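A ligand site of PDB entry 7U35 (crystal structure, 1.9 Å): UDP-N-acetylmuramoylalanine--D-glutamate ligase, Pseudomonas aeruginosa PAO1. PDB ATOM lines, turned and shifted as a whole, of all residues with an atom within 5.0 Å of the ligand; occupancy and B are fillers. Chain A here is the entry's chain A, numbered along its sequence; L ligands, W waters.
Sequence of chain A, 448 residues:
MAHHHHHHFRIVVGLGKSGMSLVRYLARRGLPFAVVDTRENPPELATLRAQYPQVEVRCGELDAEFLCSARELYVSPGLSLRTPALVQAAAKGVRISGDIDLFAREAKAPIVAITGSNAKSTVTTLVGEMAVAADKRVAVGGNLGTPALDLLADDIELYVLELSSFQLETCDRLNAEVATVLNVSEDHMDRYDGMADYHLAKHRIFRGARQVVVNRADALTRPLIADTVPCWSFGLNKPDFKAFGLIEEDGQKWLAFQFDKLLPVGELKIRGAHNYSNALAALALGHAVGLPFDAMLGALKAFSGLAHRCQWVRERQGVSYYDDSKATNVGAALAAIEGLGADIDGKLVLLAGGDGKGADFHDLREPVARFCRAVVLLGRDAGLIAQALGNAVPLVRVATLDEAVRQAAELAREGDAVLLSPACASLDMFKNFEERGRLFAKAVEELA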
ATOM      1  N   GLY A 116       4.261  17.307   3.375  1.00  0.00           N
ATOM      2  CA  GLY A 116       3.402  18.146   2.553  1.00  0.00           C
ATOM      3  C   GLY A 116       3.809  19.598   2.678  1.00  0.00           C
ATOM      4  O   GLY A 116       4.581  19.962   3.555  1.00  0.00           O
ATOM      5  N   SER A 117       3.327  20.443   1.753  1.00  0.00           N
ATOM      6  CA  SER A 117       3.695  21.846   1.821  1.00  0.00           C
ATOM      7  C   SER A 117       3.079  22.513   3.052  1.00  0.00           C
ATOM      8  O   SER A 117       3.722  23.334   3.706  1.00  0.00           O
ATOM      9  CB  SER A 117       3.248  22.563   0.536  1.00  0.00           C
ATOM     10  OG  SER A 117       3.960  22.080  -0.593  1.00  0.00           O
ATOM     11  N   ASN A 118       1.843  22.152   3.386  1.00  0.00           N
ATOM     12  CA  ASN A 118       1.105  22.767   4.472  1.00  0.00           C
ATOM     13  C   ASN A 118       0.264  21.689   5.123  1.00  0.00           C
ATOM     14  O   ASN A 118       0.075  20.611   4.569  1.00  0.00           O
ATOM     15  CB  ASN A 118       0.222  23.924   3.977  1.00  0.00           C
ATOM     16  CG  ASN A 118       1.013  25.123   3.485  1.00  0.00           C
ATOM     17  OD1 ASN A 118       1.700  25.790   4.253  1.00  0.00           O
ATOM     18  ND2 ASN A 118       0.871  25.450   2.187  1.00  0.00           N
ATOM     19  N   ALA A 119      -0.282  22.014   6.304  1.00  0.00           N
ATOM     20  CA  ALA A 119      -1.185  21.176   7.093  1.00  0.00           C
ATOM     21  C   ALA A 119      -0.466  20.054   7.817  1.00  0.00           C
ATOM     22  O   ALA A 119      -1.141  19.205   8.396  1.00  0.00           O
ATOM     23  CB  ALA A 119      -2.331  20.564   6.252  1.00  0.00           C
ATOM     24  N   LYS A 120       0.873  19.997   7.811  1.00  0.00           N
ATOM     25  CA  LYS A 120       1.562  18.854   8.419  1.00  0.00           C
ATOM     26  C   LYS A 120       1.286  18.763   9.912  1.00  0.00           C
ATOM     27  O   LYS A 120       0.984  17.691  10.432  1.00  0.00           O
ATOM     28  CB  LYS A 120       3.068  18.941   8.149  1.00  0.00           C
ATOM     29  CG  LYS A 120       3.477  18.729   6.690  1.00  0.00           C
ATOM     30  CD  LYS A 120       5.017  18.877   6.531  1.00  0.00           C
ATOM     31  CE  LYS A 120       5.536  20.256   6.939  1.00  0.00           C
ATOM     32  NZ  LYS A 120       5.033  21.399   6.109  1.00  0.00           N
ATOM     33  N   SER A 121       1.479  19.870  10.634  1.00  0.00           N
ATOM     34  CA  SER A 121       1.320  19.808  12.080  1.00  0.00           C
ATOM     35  C   SER A 121      -0.144  19.637  12.451  1.00  0.00           C
ATOM     36  O   SER A 121      -0.447  18.920  13.396  1.00  0.00           O
ATOM     37  CB  SER A 121       1.933  21.026  12.764  1.00  0.00           C
ATOM     38  OG  SER A 121       1.375  22.256  12.312  1.00  0.00           O
ATOM     39  N   THR A 122      -1.077  20.237  11.681  1.00  0.00           N
ATOM     40  CA  THR A 122      -2.498  20.012  11.969  1.00  0.00           C
ATOM     41  C   THR A 122      -2.849  18.527  11.889  1.00  0.00           C
ATOM     42  O   THR A 122      -3.461  17.960  12.801  1.00  0.00           O
ATOM     43  CB  THR A 122      -3.364  20.815  10.990  1.00  0.00           C
ATOM     44  OG1 THR A 122      -3.185  22.226  11.186  1.00  0.00           O
ATOM     45  CG2 THR A 122      -4.861  20.457  11.201  1.00  0.00           C
ATOM     46  N   GLU A 162       5.957  13.765  11.669  1.00  0.00           N
ATOM     47  CA  GLU A 162       5.875  14.824  10.671  1.00  0.00           C
ATOM     48  C   GLU A 162       7.292  15.010  10.125  1.00  0.00           C
ATOM     49  O   GLU A 162       8.243  15.090  10.908  1.00  0.00           O
ATOM     50  CB  GLU A 162       5.357  16.121  11.318  1.00  0.00           C
ATOM     51  CG  GLU A 162       5.399  17.361  10.436  1.00  0.00           C
ATOM     52  CD  GLU A 162       5.151  18.631  11.226  1.00  0.00           C
ATOM     53  OE1 GLU A 162       4.554  18.542  12.314  1.00  0.00           O
ATOM     54  OE2 GLU A 162       5.569  19.724  10.762  1.00  0.00           O
ATOM     55  N   ASN A 183      -0.192  17.678   0.409  1.00  0.00           N
ATOM     56  CA  ASN A 183      -0.409  18.637  -0.656  1.00  0.00           C
ATOM     57  C   ASN A 183       0.954  19.126  -1.114  1.00  0.00           C
ATOM     58  O   ASN A 183       1.957  18.969  -0.405  1.00  0.00           O
ATOM     59  CB  ASN A 183      -1.299  19.796  -0.180  1.00  0.00           C
ATOM     60  CG  ASN A 183      -0.818  20.378   1.140  1.00  0.00           C
ATOM     61  OD1 ASN A 183       0.206  21.053   1.195  1.00  0.00           O
ATOM     62  ND2 ASN A 183      -1.545  20.079   2.215  1.00  0.00           N
ATOM     63  N   HIS A 274     -10.820  23.371   4.297  1.00  0.00           N
ATOM     64  CA  HIS A 274      -9.439  22.873   4.330  1.00  0.00           C
ATOM     65  C   HIS A 274      -9.205  22.068   5.609  1.00  0.00           C
ATOM     66  O   HIS A 274      -8.503  21.046   5.595  1.00  0.00           O
ATOM     67  CB  HIS A 274      -8.440  24.033   4.212  1.00  0.00           C
ATOM     68  CG  HIS A 274      -8.502  24.998   5.357  1.00  0.00           C
ATOM     69  ND1 HIS A 274      -9.656  25.661   5.711  1.00  0.00           N
ATOM     70  CD2 HIS A 274      -7.545  25.401   6.233  1.00  0.00           C
ATOM     71  CE1 HIS A 274      -9.413  26.424   6.758  1.00  0.00           C
ATOM     72  NE2 HIS A 274      -8.149  26.288   7.099  1.00  0.00           N
ATOM     73  N   ASN A 275      -9.804  22.494   6.725  1.00  0.00           N
ATOM     74  CA  ASN A 275      -9.704  21.696   7.945  1.00  0.00           C
ATOM     75  C   ASN A 275     -10.594  20.450   7.882  1.00  0.00           C
ATOM     76  O   ASN A 275     -10.276  19.456   8.539  1.00  0.00           O
ATOM     77  CB  ASN A 275     -10.056  22.530   9.174  1.00  0.00           C
ATOM     78  CG  ASN A 275      -8.845  23.293   9.721  1.00  0.00           C
ATOM     79  OD1 ASN A 275      -7.723  22.799   9.723  1.00  0.00           O
ATOM     80  ND2 ASN A 275      -9.094  24.518  10.177  1.00  0.00           N
ATOM     81  N   SER A 277     -10.856  18.735   5.159  1.00  0.00           N
ATOM     82  CA  SER A 277      -9.913  17.893   4.439  1.00  0.00           C
ATOM     83  C   SER A 277      -8.850  17.330   5.372  1.00  0.00           C
ATOM     84  O   SER A 277      -8.485  16.160   5.263  1.00  0.00           O
ATOM     85  CB  SER A 277      -9.259  18.687   3.312  1.00  0.00           C
ATOM     86  OG  SER A 277      -8.243  17.920   2.686  1.00  0.00           O
ATOM     87  N   ASN A 278      -8.328  18.148   6.282  1.00  0.00           N
ATOM     88  CA  ASN A 278      -7.324  17.669   7.218  1.00  0.00           C
ATOM     89  C   ASN A 278      -7.875  16.559   8.115  1.00  0.00           C
ATOM     90  O   ASN A 278      -7.166  15.593   8.436  1.00  0.00           O
ATOM     91  CB  ASN A 278      -6.807  18.825   8.066  1.00  0.00           C
ATOM     92  CG  ASN A 278      -6.063  19.867   7.234  1.00  0.00           C
ATOM     93  OD1 ASN A 278      -5.551  19.571   6.157  1.00  0.00           O
ATOM     94  ND2 ASN A 278      -6.027  21.106   7.732  1.00  0.00           N
ATOM     95  N   HIS A 308      -3.225  29.781  15.861  1.00  0.00           N
ATOM     96  CA  HIS A 308      -3.029  30.566  14.648  1.00  0.00           C
ATOM     97  C   HIS A 308      -3.270  29.754  13.382  1.00  0.00           C
ATOM     98  O   HIS A 308      -2.889  30.181  12.293  1.00  0.00           O
ATOM     99  CB  HIS A 308      -1.631  31.210  14.628  1.00  0.00           C
ATOM    100  CG  HIS A 308      -1.225  31.780  15.945  1.00  0.00           C
ATOM    101  ND1 HIS A 308      -1.853  32.866  16.509  1.00  0.00           N
ATOM    102  CD2 HIS A 308      -0.292  31.376  16.845  1.00  0.00           C
ATOM    103  CE1 HIS A 308      -1.308  33.134  17.680  1.00  0.00           C
ATOM    104  NE2 HIS A 308      -0.358  32.239  17.911  1.00  0.00           N
ATOM    105  N   ARG A 309      -3.900  28.580  13.499  1.00  0.00           N
ATOM    106  CA  ARG A 309      -4.393  27.835  12.344  1.00  0.00           C
ATOM    107  C   ARG A 309      -5.895  28.087  12.318  1.00  0.00           C
ATOM    108  O   ARG A 309      -6.647  27.435  13.045  1.00  0.00           O
ATOM    109  CB  ARG A 309      -4.082  26.339  12.435  1.00  0.00           C
ATOM    110  CG  ARG A 309      -2.648  25.917  12.077  1.00  0.00           C
ATOM    111  CD  ARG A 309      -1.650  26.292  13.170  1.00  0.00           C
ATOM    112  NE  ARG A 309      -0.498  25.401  13.188  1.00  0.00           N
ATOM    113  CZ  ARG A 309       0.431  25.410  14.128  1.00  0.00           C
ATOM    114  NH1 ARG A 309       0.376  26.256  15.158  1.00  0.00           N
ATOM    115  NH2 ARG A 309       1.449  24.559  14.048  1.00  0.00           N
ATOM    116  N   CYS A 310      -6.301  29.080  11.536  1.00  0.00           N
ATOM    117  CA  CYS A 310      -7.702  29.508  11.344  1.00  0.00           C
ATOM    118  C   CYS A 310      -8.512  29.389  12.633  1.00  0.00           C
ATOM    119  O   CYS A 310      -9.507  28.667  12.713  1.00  0.00           O
ATOM    120  CB  CYS A 310      -8.353  28.731  10.202  1.00  0.00           C
ATOM    121  SG  CYS A 310      -9.909  29.482   9.578  1.00  0.00           S
ATOM    122  N   ASP A 324      -5.667  33.170  11.184  1.00  0.00           N
ATOM    123  CA  ASP A 324      -4.885  32.199  10.422  1.00  0.00           C
ATOM    124  C   ASP A 324      -3.507  32.759  10.131  1.00  0.00           C
ATOM    125  O   ASP A 324      -2.985  32.654   9.021  1.00  0.00           O
ATOM    126  CB  ASP A 324      -5.598  31.803   9.126  1.00  0.00           C
ATOM    127  CG  ASP A 324      -5.047  30.529   8.515  1.00  0.00           C
ATOM    128  OD1 ASP A 324      -4.794  29.557   9.272  1.00  0.00           O
ATOM    129  OD2 ASP A 324      -4.888  30.472   7.279  1.00  0.00           O
ATOM    130  N   LYS A 326      -0.692  31.731  10.706  1.00  0.00           N
ATOM    131  CA  LYS A 326       0.304  30.789  10.197  1.00  0.00           C
ATOM    132  C   LYS A 326       0.189  30.534   8.689  1.00  0.00           C
ATOM    133  O   LYS A 326       0.994  29.763   8.148  1.00  0.00           O
ATOM    134  CB  LYS A 326       0.217  29.445  10.968  1.00  0.00           C
ATOM    135  CG  LYS A 326       1.525  28.642  10.849  1.00  0.00           C
ATOM    136  CD  LYS A 326       1.678  27.565  11.899  1.00  0.00           C
ATOM    137  CE  LYS A 326       3.040  26.887  11.789  1.00  0.00           C
ATOM    138  NZ  LYS A 326       3.118  25.987  10.598  1.00  0.00           N
ATOM    139  N   ALA A 327      -0.747  31.154   7.961  1.00  0.00           N
ATOM    140  CA  ALA A 327      -0.721  31.107   6.496  1.00  0.00           C
ATOM    141  C   ALA A 327       0.383  32.029   5.979  1.00  0.00           C
ATOM    142  O   ALA A 327       0.156  33.177   5.573  1.00  0.00           O
ATOM    143  CB  ALA A 327      -2.072  31.504   5.903  1.00  0.00           C
ATOM    144  N   GLY A 331       0.057  29.056  -1.028  1.00  0.00           N
ATOM    145  CA  GLY A 331      -0.769  27.849  -1.007  1.00  0.00           C
ATOM    146  C   GLY A 331      -1.614  27.749   0.251  1.00  0.00           C
ATOM    147  O   GLY A 331      -2.785  27.321   0.198  1.00  0.00           O
ATOM    148  N   ALA A 332      -1.042  28.130   1.397  1.00  0.00           N
ATOM    149  CA  ALA A 332      -1.779  28.089   2.656  1.00  0.00           C
ATOM    150  C   ALA A 332      -2.944  29.067   2.665  1.00  0.00           C
ATOM    151  O   ALA A 332      -4.080  28.703   3.006  1.00  0.00           O
ATOM    152  CB  ALA A 332      -0.829  28.371   3.829  1.00  0.00           C
ATOM    153  N   ALA A 333      -2.694  30.316   2.274  1.00  0.00           N
ATOM    154  CA  ALA A 333      -3.762  31.304   2.263  1.00  0.00           C
ATOM    155  C   ALA A 333      -4.861  30.901   1.303  1.00  0.00           C
ATOM    156  O   ALA A 333      -6.051  31.088   1.594  1.00  0.00           O
ATOM    157  CB  ALA A 333      -3.199  32.670   1.892  1.00  0.00           C
ATOM    158  N   ALA A 335      -5.835  27.932   0.424  1.00  0.00           N
ATOM    159  CA  ALA A 335      -6.661  26.892   1.044  1.00  0.00           C
ATOM    160  C   ALA A 335      -7.568  27.459   2.129  1.00  0.00           C
ATOM    161  O   ALA A 335      -8.726  27.062   2.248  1.00  0.00           O
ATOM    162  CB  ALA A 335      -5.759  25.804   1.652  1.00  0.00           C
ATOM    163  N   ALA A 336      -7.046  28.378   2.934  1.00  0.00           N
ATOM    164  CA  ALA A 336      -7.855  28.928   4.015  1.00  0.00           C
ATOM    165  C   ALA A 336      -8.950  29.846   3.478  1.00  0.00           C
ATOM    166  O   ALA A 336     -10.057  29.910   4.045  1.00  0.00           O
ATOM    167  CB  ALA A 336      -6.968  29.678   5.009  1.00  0.00           C
ATOM    168  N   SER A 421      -5.252  35.810   7.006  1.00  0.00           N
ATOM    169  CA  SER A 421      -4.598  34.684   6.336  1.00  0.00           C
ATOM    170  C   SER A 421      -3.640  35.321   5.354  1.00  0.00           C
ATOM    171  O   SER A 421      -3.962  35.479   4.168  1.00  0.00           O
ATOM    172  CB  SER A 421      -5.613  33.780   5.626  1.00  0.00           C
ATOM    173  OG  SER A 421      -5.037  32.535   5.308  1.00  0.00           O
HETATM  174  P1  LIG L   1       2.555  22.968   8.520  1.00  0.00           P
HETATM  175  O1  LIG L   1       2.760  22.176   9.828  1.00  0.00           O
HETATM  176  O2  LIG L   1       3.342  24.305   8.461  1.00  0.00           O
HETATM  177  O3  LIG L   1       2.742  22.063   7.318  1.00  0.00           O
HETATM  178  P2  LIG L   1      -0.016  23.788   9.609  1.00  0.00           P
HETATM  179  O4  LIG L   1      -0.867  22.647  10.027  1.00  0.00           O
HETATM  180  O5  LIG L   1       0.676  24.476  10.784  1.00  0.00           O
HETATM  181  O6  LIG L   1       1.019  23.349   8.493  1.00  0.00           O
HETATM  182  O7  LIG L   1      -0.918  24.829   8.837  1.00  0.00           O
HETATM  183  C1  LIG L   1      -0.316  26.082   8.446  1.00  0.00           C
HETATM  184  C2  LIG L   1      -1.291  26.817   7.567  1.00  0.00           C
HETATM  185  O8  LIG L   1      -1.521  26.063   6.367  1.00  0.00           O
HETATM  186  C3  LIG L   1      -2.669  27.000   8.158  1.00  0.00           C
HETATM  187  O9  LIG L   1      -2.642  28.092   9.070  1.00  0.00           O
HETATM  188  C4  LIG L   1      -3.518  27.255   6.903  1.00  0.00           C
HETATM  189  O10 LIG L   1      -3.346  28.589   6.438  1.00  0.00           O
HETATM  190  C5  LIG L   1      -2.833  26.317   5.894  1.00  0.00           C
HETATM  191  N1  LIG L   1      -3.503  25.035   5.700  1.00  0.00           N
HETATM  192  C6  LIG L   1      -4.194  24.281   6.620  1.00  0.00           C
HETATM  193  N2  LIG L   1      -4.739  23.200   6.121  1.00  0.00           N
HETATM  194  C7  LIG L   1      -4.373  23.226   4.786  1.00  0.00           C
HETATM  195  C8  LIG L   1      -4.598  22.338   3.722  1.00  0.00           C
HETATM  196  N3  LIG L   1      -5.384  21.265   3.800  1.00  0.00           N
HETATM  197  N4  LIG L   1      -4.024  22.616   2.526  1.00  0.00           N
HETATM  198  C9  LIG L   1      -3.299  23.733   2.410  1.00  0.00           C
HETATM  199  N5  LIG L   1      -3.052  24.666   3.332  1.00  0.00           N
HETATM  200  C10 LIG L   1      -3.608  24.355   4.508  1.00  0.00           C
HETATM  201  O   HOH W   1      -4.546  21.735   0.049  1.00  0.00           O
HETATM  202  O   HOH W   2      -5.176  23.970   9.889  1.00  0.00           O
HETATM  203  O   HOH W   3      -3.999  18.560   2.192  1.00  0.00           O
HETATM  204  O   HOH W   4      -6.555  19.723   1.572  1.00  0.00           O
HETATM  205  O   HOH W   5       3.412  25.847   6.417  1.00  0.00           O
HETATM  206  O   HOH W   6      -6.026  26.707   9.059  1.00  0.00           O
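O of Ser 117 touches O3 of the ligand, 3.95 Å away. C of Asn 118 touches O3 of the ligand, at 3.3 Å. Glu 162 touches the ligand. Asn 183 touches the ligand. CD2 of His 274 touches C6 of the ligand, 3.6 Å away. His 308 touches the ligand. CB of Ala 327 touches O10 of the ligand, at 3.2 Å. Ala 332 touches the ligand. Ala 335 touches the ligand (CB to C9, 3.3 Å). Hydrophobic or aromatic side chains that line the ligand: Ala 119, His 274, Ala 327, Ala 332 and Ala 335. The nearest printed residue that does not touch the ligand is Ala 336 (4.04 Å).
The side-chain amino group (NZ) of Lys 120 lies within salt-bridge range of an oxygen (O3) of the ligand, 2.7 Å away. The backbone NH (N) of Ala 119 lies within hydrogen-bond range of an oxygen (O6) of the ligand, at 2.9 Å. O2 of the ligand lies within salt-bridge range of NZ of Lys 326 (2.7 Å). O1 of the ligand sits at hydrogen-bond distance from N of Ser 121, at 2.8 Å. N of Thr 122 is in hydrogen-bond range of O4 of the ligand (2.9 Å). An oxygen (O5) of the ligand lies within salt-bridge range of the guanidinium group (NE) of Arg 309 (2.8 Å). An oxygen (O10) of the ligand lies within hydrogen-bond range of the side-chain carboxylate (OD2) of Asp 324, at 2.6 Å. OG1 of Thr 122 lies within hydrogen-bond range of O4 of the ligand (2.6 Å). An oxygen (O5) of the ligand lies within hydrogen-bond range of the side-chain hydroxyl of Ser 121, 2.8 Å away. The side-chain amide oxygen of Asn 278 sits at hydrogen-bond distance from a nitrogen (N3) of the ligand, 2.9 Å away. An oxygen (O3) of the ligand lies within hydrogen-bond range of the backbone NH (N) of Lys 120 (2.8 Å).
The backbone carbonyl oxygen (O) of Gly 116 sits at hydrogen-bond distance from the side-chain amino group (NZ) of Lys 120, at 3.0 Å. The side-chain amide nitrogen (ND2) of Asn 118 lies close to the backbone NH (N) of Ala 332, 3.4 Å away. OD1 of Asp 324 is in hydrogen-bond range of N of Cys 310, at 2.8 Å. OG of Ser 421 lies within hydrogen-bond range of OD2 of Asp 324 (2.9 Å). ND2 of Asn 278 lies close to O of His 274 (3.3 Å). The side-chain hydroxyl (OG) of Ser 121 lies within hydrogen-bond range of the guanidinium group (NH2) of Arg 309, 2.9 Å away. The backbone carbonyl oxygen of His 308 is in hydrogen-bond range of the backbone NH of Lys 326, at 3.1 Å. ND2 of Asn 278 sits at hydrogen-bond distance from OD1 of Asn 275 (3.1 Å).
Water W5 lies within hydrogen-bond range of O2 of the ligand and OD1 of Asn 118. Water W4 lies within hydrogen-bond range of the side-chain hydroxyl of Ser 277 (2.7 Å) and a nitrogen (N3) of the ligand (3.0 Å). Water W6 lies within hydrogen-bond range of a ring nitrogen (NE2) of His 274 (2.9 Å), the side-chain carboxylate (OD1) of Asp 324 (3.1 Å) and the backbone NH (N) of Cys 310 (3.4 Å). Water W2 lies within hydrogen-bond range of the side-chain amide oxygen (OD1) of Asn 275 and the side-chain hydroxyl (OG1) of Thr 122. Water W3 lies within hydrogen-bond range of ND2 of Asn 183 (2.9 Å) and N3 of the ligand (3.4 Å).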
